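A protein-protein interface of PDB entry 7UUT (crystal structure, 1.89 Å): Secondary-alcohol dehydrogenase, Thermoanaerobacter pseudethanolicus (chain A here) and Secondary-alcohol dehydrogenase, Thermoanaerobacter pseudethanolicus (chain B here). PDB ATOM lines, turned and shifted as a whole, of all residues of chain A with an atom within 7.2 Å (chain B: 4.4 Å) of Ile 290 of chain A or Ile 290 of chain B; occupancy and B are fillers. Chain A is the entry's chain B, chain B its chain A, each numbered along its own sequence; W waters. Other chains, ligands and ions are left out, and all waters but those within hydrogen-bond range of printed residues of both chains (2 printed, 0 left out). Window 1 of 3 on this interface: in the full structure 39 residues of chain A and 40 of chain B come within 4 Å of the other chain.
Water W1 lies within hydrogen-bond range of O of Gly 292 of chain A (2.7 Å), N of Lys 288 of chain B (2.9 Å) and NE1 of Trp 281 of chain B (3.3 Å). Water W2 lies within hydrogen-bond range of the side-chain hydroxyl (OG1) of Thr 289 of chain B (3.1 Å) and the backbone NH (N) of Gly 292 of chain A (3.3 Å).
Of the printed residues of chain A, Ile 290 of chain B touches Trp 281 (3.8 Å), Thr 289 (3.5 Å) and Ile 290 (2.9 Å). Of the printed residues of chain A, Trp 281 of chain B touches Ile 290 and Gly 292. Of the printed residues of chain B, Gly 292 of chain A touches Trp 281 (3.9 Å). Ile 241 of chain A touches none of the printed residues of chain B. Val 253 of chain B touches none of the printed residues of chain A.
Of the 9 printed residues of chain B, 6 touch a printed residue of chain A. Hydrophobic or aromatic side chains of chain B that line the printed part of chain A: Met 249, Val 276, Trp 281 and Ile 290. Hydrophobic or aromatic side chains of chain A within 4 Å of the printed part of chain B: Val 276, Trp 281 and Ile 290. Among the printed residues, 11 pairs touch across the chains. Among the printed residues, no Asp or Glu carboxylate lies within 4 Å of a Lys or Arg side-chain nitrogen of the other chain.
Among the printed residues, pairs that only touch across the chains: Val 276 of chain A with Val 276 of chain B (3.7 Å), Trp 281 of chain A with Met 249 of chain B (3.98 Å), Trp 281 of chain A with Ile 290 of chain B (3.8 Å), Thr 289 of chain A with Thr 289 of chain B (3.6 Å), Thr 289 of chain A with Ile 290 of chain B (3.5 Å), Thr 289 of chain A with Lys 291 of chain B (3.9 Å), Ile 290 of chain A with Trp 281 of chain B (3.8 Å), Ile 290 of chain A with Thr 289 of chain B (3.6 Å), Lys 291 of chain A with Thr 289 of chain B (3.8 Å) and Gly 292 of chain A with Trp 281 of chain B (3.9 Å).
The backbone NH (N) of Ile 262 of chain A lies within hydrogen-bond range of the backbone carbonyl oxygen (O) of Thr 289 of chain A (2.6 Å). N of Ile 262 of chain B is in hydrogen-bond range of O of Thr 289 of chain B (2.6 Å). The backbone carbonyl oxygen of Ile 262 of chain A lies within hydrogen-bond range of the backbone NH of Lys 291 of chain A (2.7 Å). The backbone carbonyl oxygen of Ile 262 of chain B sits at hydrogen-bond distance from the backbone NH of Lys 291 of chain B, 2.7 Å away. The indole nitrogen (NE1) of Trp 281 of chain A lies within hydrogen-bond range of the backbone carbonyl oxygen (O) of Lys 288 of chain A. NE1 of Trp 281 of chain B lies within hydrogen-bond range of O of Lys 288 of chain B (2.9 Å).
The backbone NH (N) of Ile 290 of chain B lies within hydrogen-bond range of the backbone carbonyl oxygen (O) of Ile 290 of chain A.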
ATOM      1  N   ILE A 241      35.463  29.497  -2.850  1.00  0.00           N
ATOM      2  CA  ILE A 241      36.518  28.632  -3.366  1.00  0.00           C
ATOM      3  C   ILE A 241      37.373  29.451  -4.320  1.00  0.00           C
ATOM      4  O   ILE A 241      36.883  29.936  -5.346  1.00  0.00           O
ATOM      5  CB  ILE A 241      35.936  27.400  -4.070  1.00  0.00           C
ATOM      6  CG1 ILE A 241      35.053  26.603  -3.112  1.00  0.00           C
ATOM      7  CG2 ILE A 241      37.053  26.526  -4.606  1.00  0.00           C
ATOM      8  CD1 ILE A 241      34.408  25.405  -3.753  1.00  0.00           C
ATOM      9  N   MET A 249      35.961  21.185  -3.524  1.00  0.00           N
ATOM     10  CA  MET A 249      34.512  21.369  -3.569  1.00  0.00           C
ATOM     11  C   MET A 249      33.822  20.578  -2.464  1.00  0.00           C
ATOM     12  O   MET A 249      32.880  21.071  -1.834  1.00  0.00           O
ATOM     13  CB  MET A 249      33.981  20.957  -4.944  1.00  0.00           C
ATOM     14  CG  MET A 249      32.462  20.958  -5.069  1.00  0.00           C
ATOM     15  SD  MET A 249      31.712  22.585  -4.875  1.00  0.00           S
ATOM     16  CE  MET A 249      32.345  23.414  -6.333  1.00  0.00           C
ATOM     17  N   VAL A 253      31.404  22.177   0.784  1.00  0.00           N
ATOM     18  CA  VAL A 253      30.056  21.748   1.148  1.00  0.00           C
ATOM     19  C   VAL A 253      30.013  21.316   2.609  1.00  0.00           C
ATOM     20  O   VAL A 253      29.027  21.559   3.316  1.00  0.00           O
ATOM     21  CB  VAL A 253      29.586  20.627   0.203  1.00  0.00           C
ATOM     22  CG1 VAL A 253      28.247  20.069   0.650  1.00  0.00           C
ATOM     23  CG2 VAL A 253      29.506  21.143  -1.230  1.00  0.00           C
ATOM     24  N   GLY A 260      23.411  28.001   3.469  1.00  0.00           N
ATOM     25  CA  GLY A 260      24.511  28.840   3.050  1.00  0.00           C
ATOM     26  C   GLY A 260      24.800  28.692   1.569  1.00  0.00           C
ATOM     27  O   GLY A 260      24.085  28.023   0.821  1.00  0.00           O
ATOM     28  N   THR A 261      25.888  29.331   1.144  1.00  0.00           N
ATOM     29  CA  THR A 261      26.259  29.381  -0.262  1.00  0.00           C
ATOM     30  C   THR A 261      27.727  29.022  -0.433  1.00  0.00           C
ATOM     31  O   THR A 261      28.584  29.487   0.324  1.00  0.00           O
ATOM     32  CB  THR A 261      25.988  30.773  -0.859  1.00  0.00           C
ATOM     33  OG1 THR A 261      24.610  31.111  -0.672  1.00  0.00           O
ATOM     34  CG2 THR A 261      26.309  30.797  -2.348  1.00  0.00           C
ATOM     35  N   ILE A 262      28.009  28.187  -1.428  1.00  0.00           N
ATOM     36  CA  ILE A 262      29.369  27.923  -1.883  1.00  0.00           C
ATOM     37  C   ILE A 262      29.568  28.704  -3.177  1.00  0.00           C
ATOM     38  O   ILE A 262      28.915  28.425  -4.188  1.00  0.00           O
ATOM     39  CB  ILE A 262      29.628  26.424  -2.093  1.00  0.00           C
ATOM     40  CG1 ILE A 262      29.605  25.660  -0.762  1.00  0.00           C
ATOM     41  CG2 ILE A 262      30.960  26.211  -2.795  1.00  0.00           C
ATOM     42  CD1 ILE A 262      28.251  25.096  -0.386  1.00  0.00           C
ATOM     43  N   ALA A 263      30.469  29.683  -3.151  1.00  0.00           N
ATOM     44  CA  ALA A 263      30.777  30.513  -4.312  1.00  0.00           C
ATOM     45  C   ALA A 263      32.159  30.141  -4.830  1.00  0.00           C
ATOM     46  O   ALA A 263      33.153  30.296  -4.114  1.00  0.00           O
ATOM     47  CB  ALA A 263      30.721  31.997  -3.961  1.00  0.00           C
ATOM     48  N   ASN A 264      32.221  29.639  -6.059  1.00  0.00           N
ATOM     49  CA  ASN A 264      33.473  29.209  -6.664  1.00  0.00           C
ATOM     50  C   ASN A 264      33.923  30.199  -7.729  1.00  0.00           C
ATOM     51  O   ASN A 264      33.136  30.586  -8.598  1.00  0.00           O
ATOM     52  CB  ASN A 264      33.342  27.819  -7.282  1.00  0.00           C
ATOM     53  CG  ASN A 264      34.567  27.430  -8.076  1.00  0.00           C
ATOM     54  OD1 ASN A 264      35.633  27.188  -7.512  1.00  0.00           O
ATOM     55  ND2 ASN A 264      34.427  27.375  -9.394  1.00  0.00           N
ATOM     56  N   PRO A 275      33.447  16.790  -7.236  1.00  0.00           N
ATOM     57  CA  PRO A 275      32.628  15.985  -6.316  1.00  0.00           C
ATOM     58  C   PRO A 275      31.800  16.850  -5.377  1.00  0.00           C
ATOM     59  O   PRO A 275      32.310  17.790  -4.763  1.00  0.00           O
ATOM     60  CB  PRO A 275      33.671  15.169  -5.542  1.00  0.00           C
ATOM     61  CG  PRO A 275      34.883  16.043  -5.543  1.00  0.00           C
ATOM     62  CD  PRO A 275      34.873  16.775  -6.866  1.00  0.00           C
ATOM     63  N   VAL A 276      30.515  16.524  -5.267  1.00  0.00           N
ATOM     64  CA  VAL A 276      29.610  17.108  -4.286  1.00  0.00           C
ATOM     65  C   VAL A 276      29.185  15.993  -3.329  1.00  0.00           C
ATOM     66  O   VAL A 276      28.513  15.042  -3.755  1.00  0.00           O
ATOM     67  CB  VAL A 276      28.392  17.766  -4.952  1.00  0.00           C
ATOM     68  CG1 VAL A 276      27.398  18.228  -3.896  1.00  0.00           C
ATOM     69  CG2 VAL A 276      28.829  18.931  -5.828  1.00  0.00           C
ATOM     70  N   PRO A 277      29.551  16.056  -2.047  1.00  0.00           N
ATOM     71  CA  PRO A 277      29.223  14.953  -1.130  1.00  0.00           C
ATOM     72  C   PRO A 277      27.720  14.867  -0.910  1.00  0.00           C
ATOM     73  O   PRO A 277      27.072  15.867  -0.596  1.00  0.00           O
ATOM     74  CB  PRO A 277      29.959  15.326   0.165  1.00  0.00           C
ATOM     75  CG  PRO A 277      30.883  16.454  -0.199  1.00  0.00           C
ATOM     76  CD  PRO A 277      30.245  17.155  -1.356  1.00  0.00           C
ATOM     77  N   TRP A 281      25.614  17.401   1.586  1.00  0.00           N
ATOM     78  CA  TRP A 281      24.731  18.284   0.837  1.00  0.00           C
ATOM     79  C   TRP A 281      23.264  18.045   1.174  1.00  0.00           C
ATOM     80  O   TRP A 281      22.385  18.436   0.397  1.00  0.00           O
ATOM     81  CB  TRP A 281      24.973  18.117  -0.665  1.00  0.00           C
ATOM     82  CG  TRP A 281      24.611  19.317  -1.494  1.00  0.00           C
ATOM     83  CD1 TRP A 281      24.997  20.608  -1.282  1.00  0.00           C
ATOM     84  CD2 TRP A 281      23.824  19.327  -2.691  1.00  0.00           C
ATOM     85  NE1 TRP A 281      24.482  21.426  -2.260  1.00  0.00           N
ATOM     86  CE2 TRP A 281      23.760  20.662  -3.140  1.00  0.00           C
ATOM     87  CE3 TRP A 281      23.163  18.337  -3.425  1.00  0.00           C
ATOM     88  CZ2 TRP A 281      23.059  21.032  -4.284  1.00  0.00           C
ATOM     89  CZ3 TRP A 281      22.466  18.707  -4.559  1.00  0.00           C
ATOM     90  CH2 TRP A 281      22.420  20.044  -4.978  1.00  0.00           C
ATOM     91  N   HIS A 287      19.776  23.017   1.079  1.00  0.00           N
ATOM     92  CA  HIS A 287      19.748  24.426   0.680  1.00  0.00           C
ATOM     93  C   HIS A 287      21.153  25.023   0.638  1.00  0.00           C
ATOM     94  O   HIS A 287      21.346  26.212   0.896  1.00  0.00           O
ATOM     95  CB  HIS A 287      18.834  25.250   1.592  1.00  0.00           C
ATOM     96  CG  HIS A 287      17.376  25.103   1.282  1.00  0.00           C
ATOM     97  ND1 HIS A 287      16.574  24.159   1.889  1.00  0.00           N
ATOM     98  CD2 HIS A 287      16.570  25.795   0.442  1.00  0.00           C
ATOM     99  CE1 HIS A 287      15.339  24.273   1.432  1.00  0.00           C
ATOM    100  NE2 HIS A 287      15.311  25.256   0.550  1.00  0.00           N
ATOM    101  N   LYS A 288      22.150  24.201   0.315  1.00  0.00           N
ATOM    102  CA  LYS A 288      23.518  24.681   0.137  1.00  0.00           C
ATOM    103  C   LYS A 288      23.703  25.009  -1.338  1.00  0.00           C
ATOM    104  O   LYS A 288      23.979  24.128  -2.154  1.00  0.00           O
ATOM    105  CB  LYS A 288      24.533  23.651   0.617  1.00  0.00           C
ATOM    106  CG  LYS A 288      24.462  23.375   2.104  1.00  0.00           C
ATOM    107  CD  LYS A 288      25.595  22.477   2.555  1.00  0.00           C
ATOM    108  CE  LYS A 288      25.389  22.041   3.991  1.00  0.00           C
ATOM    109  NZ  LYS A 288      26.505  21.188   4.473  1.00  0.00           N
ATOM    110  N   THR A 289      23.534  26.282  -1.682  1.00  0.00           N
ATOM    111  CA  THR A 289      23.649  26.719  -3.065  1.00  0.00           C
ATOM    112  C   THR A 289      25.106  26.707  -3.511  1.00  0.00           C
ATOM    113  O   THR A 289      25.999  27.139  -2.776  1.00  0.00           O
ATOM    114  CB  THR A 289      23.072  28.127  -3.224  1.00  0.00           C
ATOM    115  OG1 THR A 289      21.694  28.129  -2.835  1.00  0.00           O
ATOM    116  CG2 THR A 289      23.169  28.579  -4.664  1.00  0.00           C
ATOM    117  N   ILE A 290      25.345  26.198  -4.718  1.00  0.00           N
ATOM    118  CA  ILE A 290      26.675  26.171  -5.316  1.00  0.00           C
ATOM    119  C   ILE A 290      26.659  27.075  -6.541  1.00  0.00           C
ATOM    120  O   ILE A 290      25.916  26.821  -7.497  1.00  0.00           O
ATOM    121  CB  ILE A 290      27.102  24.744  -5.694  1.00  0.00           C
ATOM    122  CG1 ILE A 290      27.029  23.823  -4.476  1.00  0.00           C
ATOM    123  CG2 ILE A 290      28.497  24.747  -6.302  1.00  0.00           C
ATOM    124  CD1 ILE A 290      27.283  22.367  -4.800  1.00  0.00           C
ATOM    125  N   LYS A 291      27.478  28.126  -6.512  1.00  0.00           N
ATOM    126  CA  LYS A 291      27.637  29.043  -7.630  1.00  0.00           C
ATOM    127  C   LYS A 291      29.080  29.022  -8.116  1.00  0.00           C
ATOM    128  O   LYS A 291      30.013  28.838  -7.329  1.00  0.00           O
ATOM    129  CB  LYS A 291      27.259  30.472  -7.241  1.00  0.00           C
ATOM    130  CG  LYS A 291      25.819  30.663  -6.794  1.00  0.00           C
ATOM    131  CD  LYS A 291      25.586  32.118  -6.448  1.00  0.00           C
ATOM    132  CE  LYS A 291      24.197  32.360  -5.904  1.00  0.00           C
ATOM    133  NZ  LYS A 291      24.063  33.777  -5.473  1.00  0.00           N
ATOM    134  N   GLY A 292      29.260  29.234  -9.416  1.00  0.00           N
ATOM    135  CA  GLY A 292      30.590  29.315  -9.988  1.00  0.00           C
ATOM    136  C   GLY A 292      30.615  30.154 -11.247  1.00  0.00           C
ATOM    137  O   GLY A 292      29.992  29.778 -12.242  1.00  0.00           O
ATOM    138  N   MET B 249      22.491  14.653 -12.101  1.00  0.00           N
ATOM    139  CA  MET B 249      23.079  15.962 -11.843  1.00  0.00           C
ATOM    140  C   MET B 249      23.986  16.381 -12.991  1.00  0.00           C
ATOM    141  O   MET B 249      23.982  17.545 -13.406  1.00  0.00           O
ATOM    142  CB  MET B 249      23.856  15.941 -10.528  1.00  0.00           C
ATOM    143  CG  MET B 249      24.616  17.222 -10.227  1.00  0.00           C
ATOM    144  SD  MET B 249      23.527  18.640  -9.994  1.00  0.00           S
ATOM    145  CE  MET B 249      22.683  18.150  -8.489  1.00  0.00           C
ATOM    146  N   VAL B 253      23.486  19.733 -15.546  1.00  0.00           N
ATOM    147  CA  VAL B 253      24.513  20.730 -15.829  1.00  0.00           C
ATOM    148  C   VAL B 253      24.743  20.845 -17.331  1.00  0.00           C
ATOM    149  O   VAL B 253      24.964  21.941 -17.861  1.00  0.00           O
ATOM    150  CB  VAL B 253      25.810  20.374 -15.076  1.00  0.00           C
ATOM    151  CG1 VAL B 253      26.938  21.318 -15.462  1.00  0.00           C
ATOM    152  CG2 VAL B 253      25.573  20.395 -13.570  1.00  0.00           C
ATOM    153  N   ILE B 262      20.207  25.044 -11.909  1.00  0.00           N
ATOM    154  CA  ILE B 262      19.800  23.665 -11.666  1.00  0.00           C
ATOM    155  C   ILE B 262      19.150  23.616 -10.289  1.00  0.00           C
ATOM    156  O   ILE B 262      19.807  23.873  -9.273  1.00  0.00           O
ATOM    157  CB  ILE B 262      20.990  22.693 -11.745  1.00  0.00           C
ATOM    158  CG1 ILE B 262      21.550  22.616 -13.168  1.00  0.00           C
ATOM    159  CG2 ILE B 262      20.574  21.311 -11.288  1.00  0.00           C
ATOM    160  CD1 ILE B 262      22.663  23.603 -13.442  1.00  0.00           C
ATOM    161  N   VAL B 276      29.490  16.656 -10.686  1.00  0.00           N
ATOM    162  CA  VAL B 276      29.341  17.901 -11.431  1.00  0.00           C
ATOM    163  C   VAL B 276      30.404  17.905 -12.527  1.00  0.00           C
ATOM    164  O   VAL B 276      31.604  17.963 -12.220  1.00  0.00           O
ATOM    165  CB  VAL B 276      29.469  19.130 -10.521  1.00  0.00           C
ATOM    166  CG1 VAL B 276      29.471  20.402 -11.350  1.00  0.00           C
ATOM    167  CG2 VAL B 276      28.339  19.157  -9.508  1.00  0.00           C
ATOM    168  N   TRP B 281      30.447  22.469 -16.777  1.00  0.00           N
ATOM    169  CA  TRP B 281      30.214  23.519 -15.798  1.00  0.00           C
ATOM    170  C   TRP B 281      31.144  24.709 -15.998  1.00  0.00           C
ATOM    171  O   TRP B 281      31.325  25.511 -15.074  1.00  0.00           O
ATOM    172  CB  TRP B 281      30.361  22.956 -14.381  1.00  0.00           C
ATOM    173  CG  TRP B 281      29.600  23.704 -13.340  1.00  0.00           C
ATOM    174  CD1 TRP B 281      28.279  24.047 -13.378  1.00  0.00           C
ATOM    175  CD2 TRP B 281      30.103  24.180 -12.088  1.00  0.00           C
ATOM    176  NE1 TRP B 281      27.932  24.720 -12.230  1.00  0.00           N
ATOM    177  CE2 TRP B 281      29.034  24.814 -11.422  1.00  0.00           C
ATOM    178  CE3 TRP B 281      31.354  24.135 -11.466  1.00  0.00           C
ATOM    179  CZ2 TRP B 281      29.180  25.401 -10.166  1.00  0.00           C
ATOM    180  CZ3 TRP B 281      31.498  24.720 -10.220  1.00  0.00           C
ATOM    181  CH2 TRP B 281      30.418  25.344  -9.583  1.00  0.00           C
ATOM    182  N   LYS B 288      26.448  28.549 -13.744  1.00  0.00           N
ATOM    183  CA  LYS B 288      25.338  27.602 -13.631  1.00  0.00           C
ATOM    184  C   LYS B 288      25.086  27.328 -12.149  1.00  0.00           C
ATOM    185  O   LYS B 288      25.784  26.523 -11.526  1.00  0.00           O
ATOM    186  CB  LYS B 288      25.647  26.323 -14.402  1.00  0.00           C
ATOM    187  CG  LYS B 288      25.798  26.541 -15.903  1.00  0.00           C
ATOM    188  CD  LYS B 288      25.959  25.233 -16.661  1.00  0.00           C
ATOM    189  CE  LYS B 288      26.326  25.495 -18.114  1.00  0.00           C
ATOM    190  NZ  LYS B 288      26.484  24.237 -18.904  1.00  0.00           N
ATOM    191  N   THR B 289      24.104  28.020 -11.575  1.00  0.00           N
ATOM    192  CA  THR B 289      23.793  27.867 -10.158  1.00  0.00           C
ATOM    193  C   THR B 289      23.110  26.529  -9.885  1.00  0.00           C
ATOM    194  O   THR B 289      22.216  26.106 -10.623  1.00  0.00           O
ATOM    195  CB  THR B 289      22.905  29.019  -9.687  1.00  0.00           C
ATOM    196  OG1 THR B 289      23.590  30.262  -9.883  1.00  0.00           O
ATOM    197  CG2 THR B 289      22.564  28.876  -8.216  1.00  0.00           C
ATOM    198  N   ILE B 290      23.546  25.855  -8.823  1.00  0.00           N
ATOM    199  CA  ILE B 290      22.984  24.575  -8.403  1.00  0.00           C
ATOM    200  C   ILE B 290      22.340  24.757  -7.033  1.00  0.00           C
ATOM    201  O   ILE B 290      23.025  25.098  -6.062  1.00  0.00           O
ATOM    202  CB  ILE B 290      24.052  23.469  -8.362  1.00  0.00           C
ATOM    203  CG1 ILE B 290      24.771  23.374  -9.708  1.00  0.00           C
ATOM    204  CG2 ILE B 290      23.420  22.136  -8.022  1.00  0.00           C
ATOM    205  CD1 ILE B 290      25.946  22.425  -9.707  1.00  0.00           C
ATOM    206  N   LYS B 291      21.033  24.518  -6.952  1.00  0.00           N
ATOM    207  CA  LYS B 291      20.295  24.588  -5.700  1.00  0.00           C
ATOM    208  C   LYS B 291      19.685  23.232  -5.372  1.00  0.00           C
ATOM    209  O   LYS B 291      19.317  22.464  -6.265  1.00  0.00           O
ATOM    210  CB  LYS B 291      19.178  25.634  -5.762  1.00  0.00           C
ATOM    211  CG  LYS B 291      19.641  27.055  -6.023  1.00  0.00           C
ATOM    212  CD  LYS B 291      18.443  27.985  -6.063  1.00  0.00           C
ATOM    213  CE  LYS B 291      18.831  29.406  -6.430  1.00  0.00           C
ATOM    214  NZ  LYS B 291      17.622  30.268  -6.570  1.00  0.00           N
HETATM  215  O   HOH W   1      29.156  27.484 -13.447  1.00  0.00           O
HETATM  216  O   HOH W   2      26.602  30.776 -10.601  1.00  0.00           O
